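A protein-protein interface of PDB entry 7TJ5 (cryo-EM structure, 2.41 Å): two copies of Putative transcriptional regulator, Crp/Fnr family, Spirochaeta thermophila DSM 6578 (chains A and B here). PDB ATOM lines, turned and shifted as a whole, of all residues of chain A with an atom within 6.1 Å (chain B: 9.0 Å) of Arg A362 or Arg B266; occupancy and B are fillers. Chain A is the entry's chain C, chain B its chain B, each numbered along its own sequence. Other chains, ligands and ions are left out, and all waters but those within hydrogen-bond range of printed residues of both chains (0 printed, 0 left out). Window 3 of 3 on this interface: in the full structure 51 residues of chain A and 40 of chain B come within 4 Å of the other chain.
The backbone carbonyl oxygen (O) of Tyr B264 sits at hydrogen-bond distance from the guanidinium group (NH2) of Arg A362, 3.5 Å away.
OD2 of Asp A407 is in hydrogen-bond range of OH of Tyr B264 (3.2 Å).
NZ of Lys B265 lies within salt-bridge range of OD2 of Asp A407 (3.7 Å).
The side-chain carboxylate (OE1) of Glu A309 lies within hydrogen-bond range of the side-chain hydroxyl (OG) of Ser B268 (2.8 Å).
The guanidinium group of Arg A362 sits close to the guanidinium group of Arg B266 (3.3 Å).
The backbone carbonyl oxygen of Leu B262 is in hydrogen-bond range of the backbone NH of Ile B267, 3.2 Å away.
OE1 of Gln B272 lies close to O of Ile B267 (3.4 Å).
Tyr A281 touches Tyr B264.
Glu A309 touches Ile B267.
Glu A309 touches Leu B271.
Lys B265 touches Asn A361 (NZ to OD1, 3.7 Å).
Printed residues of chain B within 4 Å of Tyr A281: Tyr B264 (3.8 Å).
Printed residues of chain B within 4 Å of Glu A309: Ile B267 (3.2 Å), Ser B268 (2.8 Å) and Leu B271 (3.3 Å).
Ile A360 touches none of the printed residues of chain B.
Of chain B, only Tyr B264 (3.5 Å) and Arg B266 (3.3 Å) come within 4 Å of Arg A362.
No residue of chain B comes within 4 Å of Gly A363.
Ala B260 touches none of the printed residues of chain A.
Of chain A, only Arg A362 comes within 4 Å of Arg B266.
Printed residues of chain A within 4 Å of Ser B268: Glu A309 (2.8 Å).
Printed residues of chain A within 4 Å of Leu B271: Glu A309 (3.3 Å).
The nearest residue of chain B that does not touch Arg A362 is Lys B265 (4.3 Å).
The nearest residue of chain A that does not touch Arg B266 is Glu A381 (4.1 Å).
The nearest printed residue of chain B that does not touch Asn A361 is Arg B266 (5.0 Å).
Of the 13 printed residues of chain B, 6 touch a printed residue of chain A.
Hydrophobic or aromatic side chains of chain A that line the printed part of chain B: Tyr A281.
Along chain A the printed residues that touch a printed residue of chain B span positions 281 to 407.
Among the printed residues, Asp or Glu carboxylates within 4 Å of a Lys or Arg side-chain nitrogen of the other chain: Asp A407 with Lys B265 (3.7 Å).
No position is printed for both chains.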
ATOM      1  N   TYR A 281      20.444  33.489  11.823  1.00  0.00           N
ATOM      2  CA  TYR A 281      19.211  33.459  12.606  1.00  0.00           C
ATOM      3  C   TYR A 281      18.881  32.040  13.048  1.00  0.00           C
ATOM      4  O   TYR A 281      18.391  31.824  14.165  1.00  0.00           O
ATOM      5  CB  TYR A 281      18.063  34.048  11.783  1.00  0.00           C
ATOM      6  CG  TYR A 281      16.676  33.733  12.299  1.00  0.00           C
ATOM      7  CD1 TYR A 281      16.106  34.481  13.320  1.00  0.00           C
ATOM      8  CD2 TYR A 281      15.930  32.693  11.756  1.00  0.00           C
ATOM      9  CE1 TYR A 281      14.838  34.202  13.788  1.00  0.00           C
ATOM     10  CE2 TYR A 281      14.662  32.403  12.222  1.00  0.00           C
ATOM     11  CZ  TYR A 281      14.122  33.160  13.240  1.00  0.00           C
ATOM     12  OH  TYR A 281      12.859  32.879  13.704  1.00  0.00           O
ATOM     13  N   GLU A 309       0.481  19.829  20.500  1.00  0.00           N
ATOM     14  CA  GLU A 309       0.816  20.903  21.427  1.00  0.00           C
ATOM     15  C   GLU A 309       1.361  22.133  20.715  1.00  0.00           C
ATOM     16  O   GLU A 309       1.294  23.233  21.268  1.00  0.00           O
ATOM     17  CB  GLU A 309       1.830  20.413  22.460  1.00  0.00           C
ATOM     18  CG  GLU A 309       1.360  20.558  23.896  1.00  0.00           C
ATOM     19  CD  GLU A 309       2.150  19.694  24.853  1.00  0.00           C
ATOM     20  OE1 GLU A 309       3.389  19.833  24.894  1.00  0.00           O
ATOM     21  OE2 GLU A 309       1.533  18.875  25.567  1.00  0.00           O
ATOM     22  N   ILE A 360       0.710  31.122  10.866  1.00  0.00           N
ATOM     23  CA  ILE A 360       1.794  31.868  11.498  1.00  0.00           C
ATOM     24  C   ILE A 360       2.087  31.263  12.865  1.00  0.00           C
ATOM     25  O   ILE A 360       1.176  31.056  13.673  1.00  0.00           O
ATOM     26  CB  ILE A 360       1.430  33.354  11.619  1.00  0.00           C
ATOM     27  CG1 ILE A 360       1.179  33.953  10.234  1.00  0.00           C
ATOM     28  CG2 ILE A 360       2.527  34.110  12.358  1.00  0.00           C
ATOM     29  CD1 ILE A 360       1.314  35.455  10.176  1.00  0.00           C
ATOM     30  N   ASN A 361       3.360  30.979  13.125  1.00  0.00           N
ATOM     31  CA  ASN A 361       3.784  30.400  14.395  1.00  0.00           C
ATOM     32  C   ASN A 361       4.632  31.335  15.241  1.00  0.00           C
ATOM     33  O   ASN A 361       4.432  31.405  16.456  1.00  0.00           O
ATOM     34  CB  ASN A 361       4.566  29.103  14.148  1.00  0.00           C
ATOM     35  CG  ASN A 361       4.530  28.165  15.337  1.00  0.00           C
ATOM     36  OD1 ASN A 361       5.525  27.999  16.041  1.00  0.00           O
ATOM     37  ND2 ASN A 361       3.379  27.547  15.569  1.00  0.00           N
ATOM     38  N   ARG A 362       5.572  32.053  14.640  1.00  0.00           N
ATOM     39  CA  ARG A 362       6.474  32.901  15.415  1.00  0.00           C
ATOM     40  C   ARG A 362       6.575  34.329  14.898  1.00  0.00           C
ATOM     41  O   ARG A 362       6.686  35.257  15.701  1.00  0.00           O
ATOM     42  CB  ARG A 362       7.876  32.265  15.456  1.00  0.00           C
ATOM     43  CG  ARG A 362       8.797  32.860  16.511  1.00  0.00           C
ATOM     44  CD  ARG A 362       8.171  32.806  17.895  1.00  0.00           C
ATOM     45  NE  ARG A 362       7.843  31.446  18.302  1.00  0.00           N
ATOM     46  CZ  ARG A 362       8.632  30.675  19.039  1.00  0.00           C
ATOM     47  NH1 ARG A 362       9.807  31.101  19.471  1.00  0.00           N
ATOM     48  NH2 ARG A 362       8.231  29.446  19.351  1.00  0.00           N
ATOM     49  N   GLY A 363       6.542  34.532  13.582  1.00  0.00           N
ATOM     50  CA  GLY A 363       6.846  35.820  12.996  1.00  0.00           C
ATOM     51  C   GLY A 363       5.638  36.731  12.867  1.00  0.00           C
ATOM     52  O   GLY A 363       4.570  36.497  13.433  1.00  0.00           O
ATOM     53  N   SER A 364       5.834  37.802  12.098  1.00  0.00           N
ATOM     54  CA  SER A 364       4.805  38.790  11.811  1.00  0.00           C
ATOM     55  C   SER A 364       4.741  39.031  10.309  1.00  0.00           C
ATOM     56  O   SER A 364       5.723  38.827   9.591  1.00  0.00           O
ATOM     57  CB  SER A 364       5.070  40.109  12.545  1.00  0.00           C
ATOM     58  OG  SER A 364       4.339  41.174  11.964  1.00  0.00           O
ATOM     59  N   SER A 380      -0.055  38.412  13.347  1.00  0.00           N
ATOM     60  CA  SER A 380       0.860  37.958  14.383  1.00  0.00           C
ATOM     61  C   SER A 380       0.630  36.468  14.640  1.00  0.00           C
ATOM     62  O   SER A 380      -0.031  35.777  13.858  1.00  0.00           O
ATOM     63  CB  SER A 380       0.680  38.790  15.655  1.00  0.00           C
ATOM     64  OG  SER A 380       1.698  38.508  16.598  1.00  0.00           O
ATOM     65  N   GLU A 381       1.211  35.974  15.733  1.00  0.00           N
ATOM     66  CA  GLU A 381       1.061  34.579  16.126  1.00  0.00           C
ATOM     67  C   GLU A 381      -0.408  34.200  16.291  1.00  0.00           C
ATOM     68  O   GLU A 381      -1.252  35.026  16.648  1.00  0.00           O
ATOM     69  CB  GLU A 381       1.799  34.310  17.437  1.00  0.00           C
ATOM     70  CG  GLU A 381       3.025  35.175  17.681  1.00  0.00           C
ATOM     71  CD  GLU A 381       4.112  34.430  18.434  1.00  0.00           C
ATOM     72  OE1 GLU A 381       3.775  33.672  19.366  1.00  0.00           O
ATOM     73  OE2 GLU A 381       5.303  34.596  18.099  1.00  0.00           O
ATOM     74  N   PHE A 405      11.944  37.413  10.309  1.00  0.00           N
ATOM     75  CA  PHE A 405      11.893  35.976  10.078  1.00  0.00           C
ATOM     76  C   PHE A 405      10.591  35.409  10.632  1.00  0.00           C
ATOM     77  O   PHE A 405      10.209  35.696  11.771  1.00  0.00           O
ATOM     78  CB  PHE A 405      13.097  35.289  10.722  1.00  0.00           C
ATOM     79  CG  PHE A 405      14.397  35.544  10.009  1.00  0.00           C
ATOM     80  CD1 PHE A 405      14.785  34.742   8.948  1.00  0.00           C
ATOM     81  CD2 PHE A 405      15.239  36.567  10.409  1.00  0.00           C
ATOM     82  CE1 PHE A 405      15.979  34.967   8.289  1.00  0.00           C
ATOM     83  CE2 PHE A 405      16.438  36.796   9.756  1.00  0.00           C
ATOM     84  CZ  PHE A 405      16.806  35.994   8.695  1.00  0.00           C
ATOM     85  N   CYS A 406       9.908  34.601   9.823  1.00  0.00           N
ATOM     86  CA  CYS A 406       8.532  34.217  10.114  1.00  0.00           C
ATOM     87  C   CYS A 406       8.445  32.890  10.866  1.00  0.00           C
ATOM     88  O   CYS A 406       7.838  32.823  11.938  1.00  0.00           O
ATOM     89  CB  CYS A 406       7.728  34.149   8.812  1.00  0.00           C
ATOM     90  SG  CYS A 406       6.866  35.683   8.406  1.00  0.00           S
ATOM     91  N   ASP A 407       9.033  31.833  10.301  1.00  0.00           N
ATOM     92  CA  ASP A 407       8.964  30.474  10.843  1.00  0.00           C
ATOM     93  C   ASP A 407       7.501  30.029  10.961  1.00  0.00           C
ATOM     94  O   ASP A 407       6.953  29.835  12.048  1.00  0.00           O
ATOM     95  CB  ASP A 407       9.707  30.389  12.186  1.00  0.00           C
ATOM     96  CG  ASP A 407       9.748  28.979  12.766  1.00  0.00           C
ATOM     97  OD1 ASP A 407       9.258  28.027  12.123  1.00  0.00           O
ATOM     98  OD2 ASP A 407      10.277  28.828  13.887  1.00  0.00           O
ATOM     99  N   LEU A 408       6.873  29.897   9.796  1.00  0.00           N
ATOM    100  CA  LEU A 408       5.458  29.574   9.697  1.00  0.00           C
ATOM    101  C   LEU A 408       5.273  28.205   9.055  1.00  0.00           C
ATOM    102  O   LEU A 408       6.167  27.678   8.394  1.00  0.00           O
ATOM    103  CB  LEU A 408       4.699  30.658   8.916  1.00  0.00           C
ATOM    104  CG  LEU A 408       5.241  31.214   7.596  1.00  0.00           C
ATOM    105  CD1 LEU A 408       4.887  30.326   6.421  1.00  0.00           C
ATOM    106  CD2 LEU A 408       4.716  32.621   7.371  1.00  0.00           C
ATOM    107  N   THR B 259      15.795  17.830  23.066  1.00  0.00           N
ATOM    108  CA  THR B 259      15.403  18.656  24.203  1.00  0.00           C
ATOM    109  C   THR B 259      15.548  20.140  23.884  1.00  0.00           C
ATOM    110  O   THR B 259      14.679  20.943  24.239  1.00  0.00           O
ATOM    111  CB  THR B 259      16.236  18.290  25.432  1.00  0.00           C
ATOM    112  OG1 THR B 259      16.124  16.884  25.683  1.00  0.00           O
ATOM    113  CG2 THR B 259      15.751  19.053  26.655  1.00  0.00           C
ATOM    114  N   ALA B 260      16.633  20.523  23.205  1.00  0.00           N
ATOM    115  CA  ALA B 260      16.818  21.922  22.830  1.00  0.00           C
ATOM    116  C   ALA B 260      15.748  22.381  21.849  1.00  0.00           C
ATOM    117  O   ALA B 260      15.211  23.494  21.974  1.00  0.00           O
ATOM    118  CB  ALA B 260      18.212  22.126  22.239  1.00  0.00           C
ATOM    119  N   PHE B 261      15.408  21.533  20.872  1.00  0.00           N
ATOM    120  CA  PHE B 261      14.376  21.916  19.917  1.00  0.00           C
ATOM    121  C   PHE B 261      13.024  22.059  20.602  1.00  0.00           C
ATOM    122  O   PHE B 261      12.251  22.966  20.273  1.00  0.00           O
ATOM    123  CB  PHE B 261      14.293  20.903  18.775  1.00  0.00           C
ATOM    124  CG  PHE B 261      13.280  21.267  17.730  1.00  0.00           C
ATOM    125  CD1 PHE B 261      13.590  22.184  16.741  1.00  0.00           C
ATOM    126  CD2 PHE B 261      12.014  20.705  17.746  1.00  0.00           C
ATOM    127  CE1 PHE B 261      12.660  22.529  15.785  1.00  0.00           C
ATOM    128  CE2 PHE B 261      11.079  21.049  16.793  1.00  0.00           C
ATOM    129  CZ  PHE B 261      11.403  21.962  15.813  1.00  0.00           C
ATOM    130  N   LEU B 262      12.712  21.169  21.549  1.00  0.00           N
ATOM    131  CA  LEU B 262      11.453  21.315  22.270  1.00  0.00           C
ATOM    132  C   LEU B 262      11.482  22.532  23.181  1.00  0.00           C
ATOM    133  O   LEU B 262      10.432  23.123  23.459  1.00  0.00           O
ATOM    134  CB  LEU B 262      11.152  20.061  23.084  1.00  0.00           C
ATOM    135  CG  LEU B 262      10.871  18.763  22.331  1.00  0.00           C
ATOM    136  CD1 LEU B 262      10.059  17.871  23.230  1.00  0.00           C
ATOM    137  CD2 LEU B 262      10.142  19.016  21.021  1.00  0.00           C
ATOM    138  N   SER B 263      12.668  22.907  23.667  1.00  0.00           N
ATOM    139  CA  SER B 263      12.792  24.120  24.463  1.00  0.00           C
ATOM    140  C   SER B 263      12.456  25.342  23.624  1.00  0.00           C
ATOM    141  O   SER B 263      11.810  26.280  24.105  1.00  0.00           O
ATOM    142  CB  SER B 263      14.202  24.231  25.043  1.00  0.00           C
ATOM    143  OG  SER B 263      15.099  24.793  24.103  1.00  0.00           O
ATOM    144  N   TYR B 264      12.904  25.352  22.363  1.00  0.00           N
ATOM    145  CA  TYR B 264      12.603  26.481  21.488  1.00  0.00           C
ATOM    146  C   TYR B 264      11.103  26.603  21.246  1.00  0.00           C
ATOM    147  O   TYR B 264      10.550  27.709  21.259  1.00  0.00           O
ATOM    148  CB  TYR B 264      13.350  26.336  20.163  1.00  0.00           C
ATOM    149  CG  TYR B 264      12.967  27.375  19.133  1.00  0.00           C
ATOM    150  CD1 TYR B 264      13.349  28.701  19.278  1.00  0.00           C
ATOM    151  CD2 TYR B 264      12.219  27.027  18.016  1.00  0.00           C
ATOM    152  CE1 TYR B 264      12.999  29.653  18.340  1.00  0.00           C
ATOM    153  CE2 TYR B 264      11.864  27.970  17.073  1.00  0.00           C
ATOM    154  CZ  TYR B 264      12.257  29.282  17.239  1.00  0.00           C
ATOM    155  OH  TYR B 264      11.905  30.223  16.300  1.00  0.00           O
ATOM    156  N   LYS B 265      10.430  25.476  21.018  1.00  0.00           N
ATOM    157  CA  LYS B 265       9.006  25.440  20.707  1.00  0.00           C
ATOM    158  C   LYS B 265       8.120  25.508  21.946  1.00  0.00           C
ATOM    159  O   LYS B 265       6.896  25.390  21.807  1.00  0.00           O
ATOM    160  CB  LYS B 265       8.676  24.182  19.900  1.00  0.00           C
ATOM    161  CG  LYS B 265       9.308  24.153  18.520  1.00  0.00           C
ATOM    162  CD  LYS B 265       8.557  25.061  17.560  1.00  0.00           C
ATOM    163  CE  LYS B 265       9.139  24.993  16.160  1.00  0.00           C
ATOM    164  NZ  LYS B 265       8.397  25.868  15.214  1.00  0.00           N
ATOM    165  N   ARG B 266       8.704  25.721  23.126  1.00  0.00           N
ATOM    166  CA  ARG B 266       7.979  25.898  24.388  1.00  0.00           C
ATOM    167  C   ARG B 266       6.970  24.770  24.616  1.00  0.00           C
ATOM    168  O   ARG B 266       5.759  24.978  24.704  1.00  0.00           O
ATOM    169  CB  ARG B 266       7.300  27.267  24.440  1.00  0.00           C
ATOM    170  CG  ARG B 266       8.267  28.435  24.568  1.00  0.00           C
ATOM    171  CD  ARG B 266       7.592  29.757  24.242  1.00  0.00           C
ATOM    172  NE  ARG B 266       7.011  29.766  22.905  1.00  0.00           N
ATOM    173  CZ  ARG B 266       6.259  30.746  22.424  1.00  0.00           C
ATOM    174  NH1 ARG B 266       5.975  31.819  23.147  1.00  0.00           N
ATOM    175  NH2 ARG B 266       5.778  30.649  21.188  1.00  0.00           N
ATOM    176  N   ILE B 267       7.505  23.558  24.706  1.00  0.00           N
ATOM    177  CA  ILE B 267       6.730  22.358  24.991  1.00  0.00           C
ATOM    178  C   ILE B 267       6.619  22.196  26.502  1.00  0.00           C
ATOM    179  O   ILE B 267       7.562  22.498  27.242  1.00  0.00           O
ATOM    180  CB  ILE B 267       7.385  21.128  24.330  1.00  0.00           C
ATOM    181  CG1 ILE B 267       7.469  21.323  22.816  1.00  0.00           C
ATOM    182  CG2 ILE B 267       6.623  19.849  24.646  1.00  0.00           C
ATOM    183  CD1 ILE B 267       6.137  21.217  22.107  1.00  0.00           C
ATOM    184  N   SER B 268       5.456  21.733  26.962  1.00  0.00           N
ATOM    185  CA  SER B 268       5.204  21.603  28.390  1.00  0.00           C
ATOM    186  C   SER B 268       6.142  20.566  29.010  1.00  0.00           C
ATOM    187  O   SER B 268       6.569  19.623  28.336  1.00  0.00           O
ATOM    188  CB  SER B 268       3.750  21.210  28.642  1.00  0.00           C
ATOM    189  OG  SER B 268       3.302  20.272  27.683  1.00  0.00           O
ATOM    190  N   PRO B 269       6.493  20.730  30.290  1.00  0.00           N
ATOM    191  CA  PRO B 269       7.426  19.784  30.926  1.00  0.00           C
ATOM    192  C   PRO B 269       6.932  18.347  30.970  1.00  0.00           C
ATOM    193  O   PRO B 269       7.758  17.430  31.039  1.00  0.00           O
ATOM    194  CB  PRO B 269       7.604  20.350  32.341  1.00  0.00           C
ATOM    195  CG  PRO B 269       7.168  21.761  32.276  1.00  0.00           C
ATOM    196  CD  PRO B 269       6.251  21.931  31.107  1.00  0.00           C
ATOM    197  N   LEU B 271       5.331  16.618  28.555  1.00  0.00           N
ATOM    198  CA  LEU B 271       5.684  15.963  27.301  1.00  0.00           C
ATOM    199  C   LEU B 271       7.188  15.738  27.200  1.00  0.00           C
ATOM    200  O   LEU B 271       7.635  14.698  26.705  1.00  0.00           O
ATOM    201  CB  LEU B 271       5.175  16.788  26.120  1.00  0.00           C
ATOM    202  CG  LEU B 271       5.162  16.112  24.749  1.00  0.00           C
ATOM    203  CD1 LEU B 271       4.709  14.665  24.858  1.00  0.00           C
ATOM    204  CD2 LEU B 271       4.263  16.882  23.803  1.00  0.00           C
ATOM    205  N   GLN B 272       7.982  16.706  27.666  1.00  0.00           N
ATOM    206  CA  GLN B 272       9.429  16.527  27.691  1.00  0.00           C
ATOM    207  C   GLN B 272       9.824  15.377  28.612  1.00  0.00           C
ATOM    208  O   GLN B 272      10.726  14.599  28.289  1.00  0.00           O
ATOM    209  CB  GLN B 272      10.112  17.825  28.122  1.00  0.00           C
ATOM    210  CG  GLN B 272       9.822  19.005  27.209  1.00  0.00           C
ATOM    211  CD  GLN B 272      10.857  20.105  27.327  1.00  0.00           C
ATOM    212  OE1 GLN B 272      10.582  21.175  27.871  1.00  0.00           O
ATOM    213  NE2 GLN B 272      12.055  19.849  26.816  1.00  0.00           N
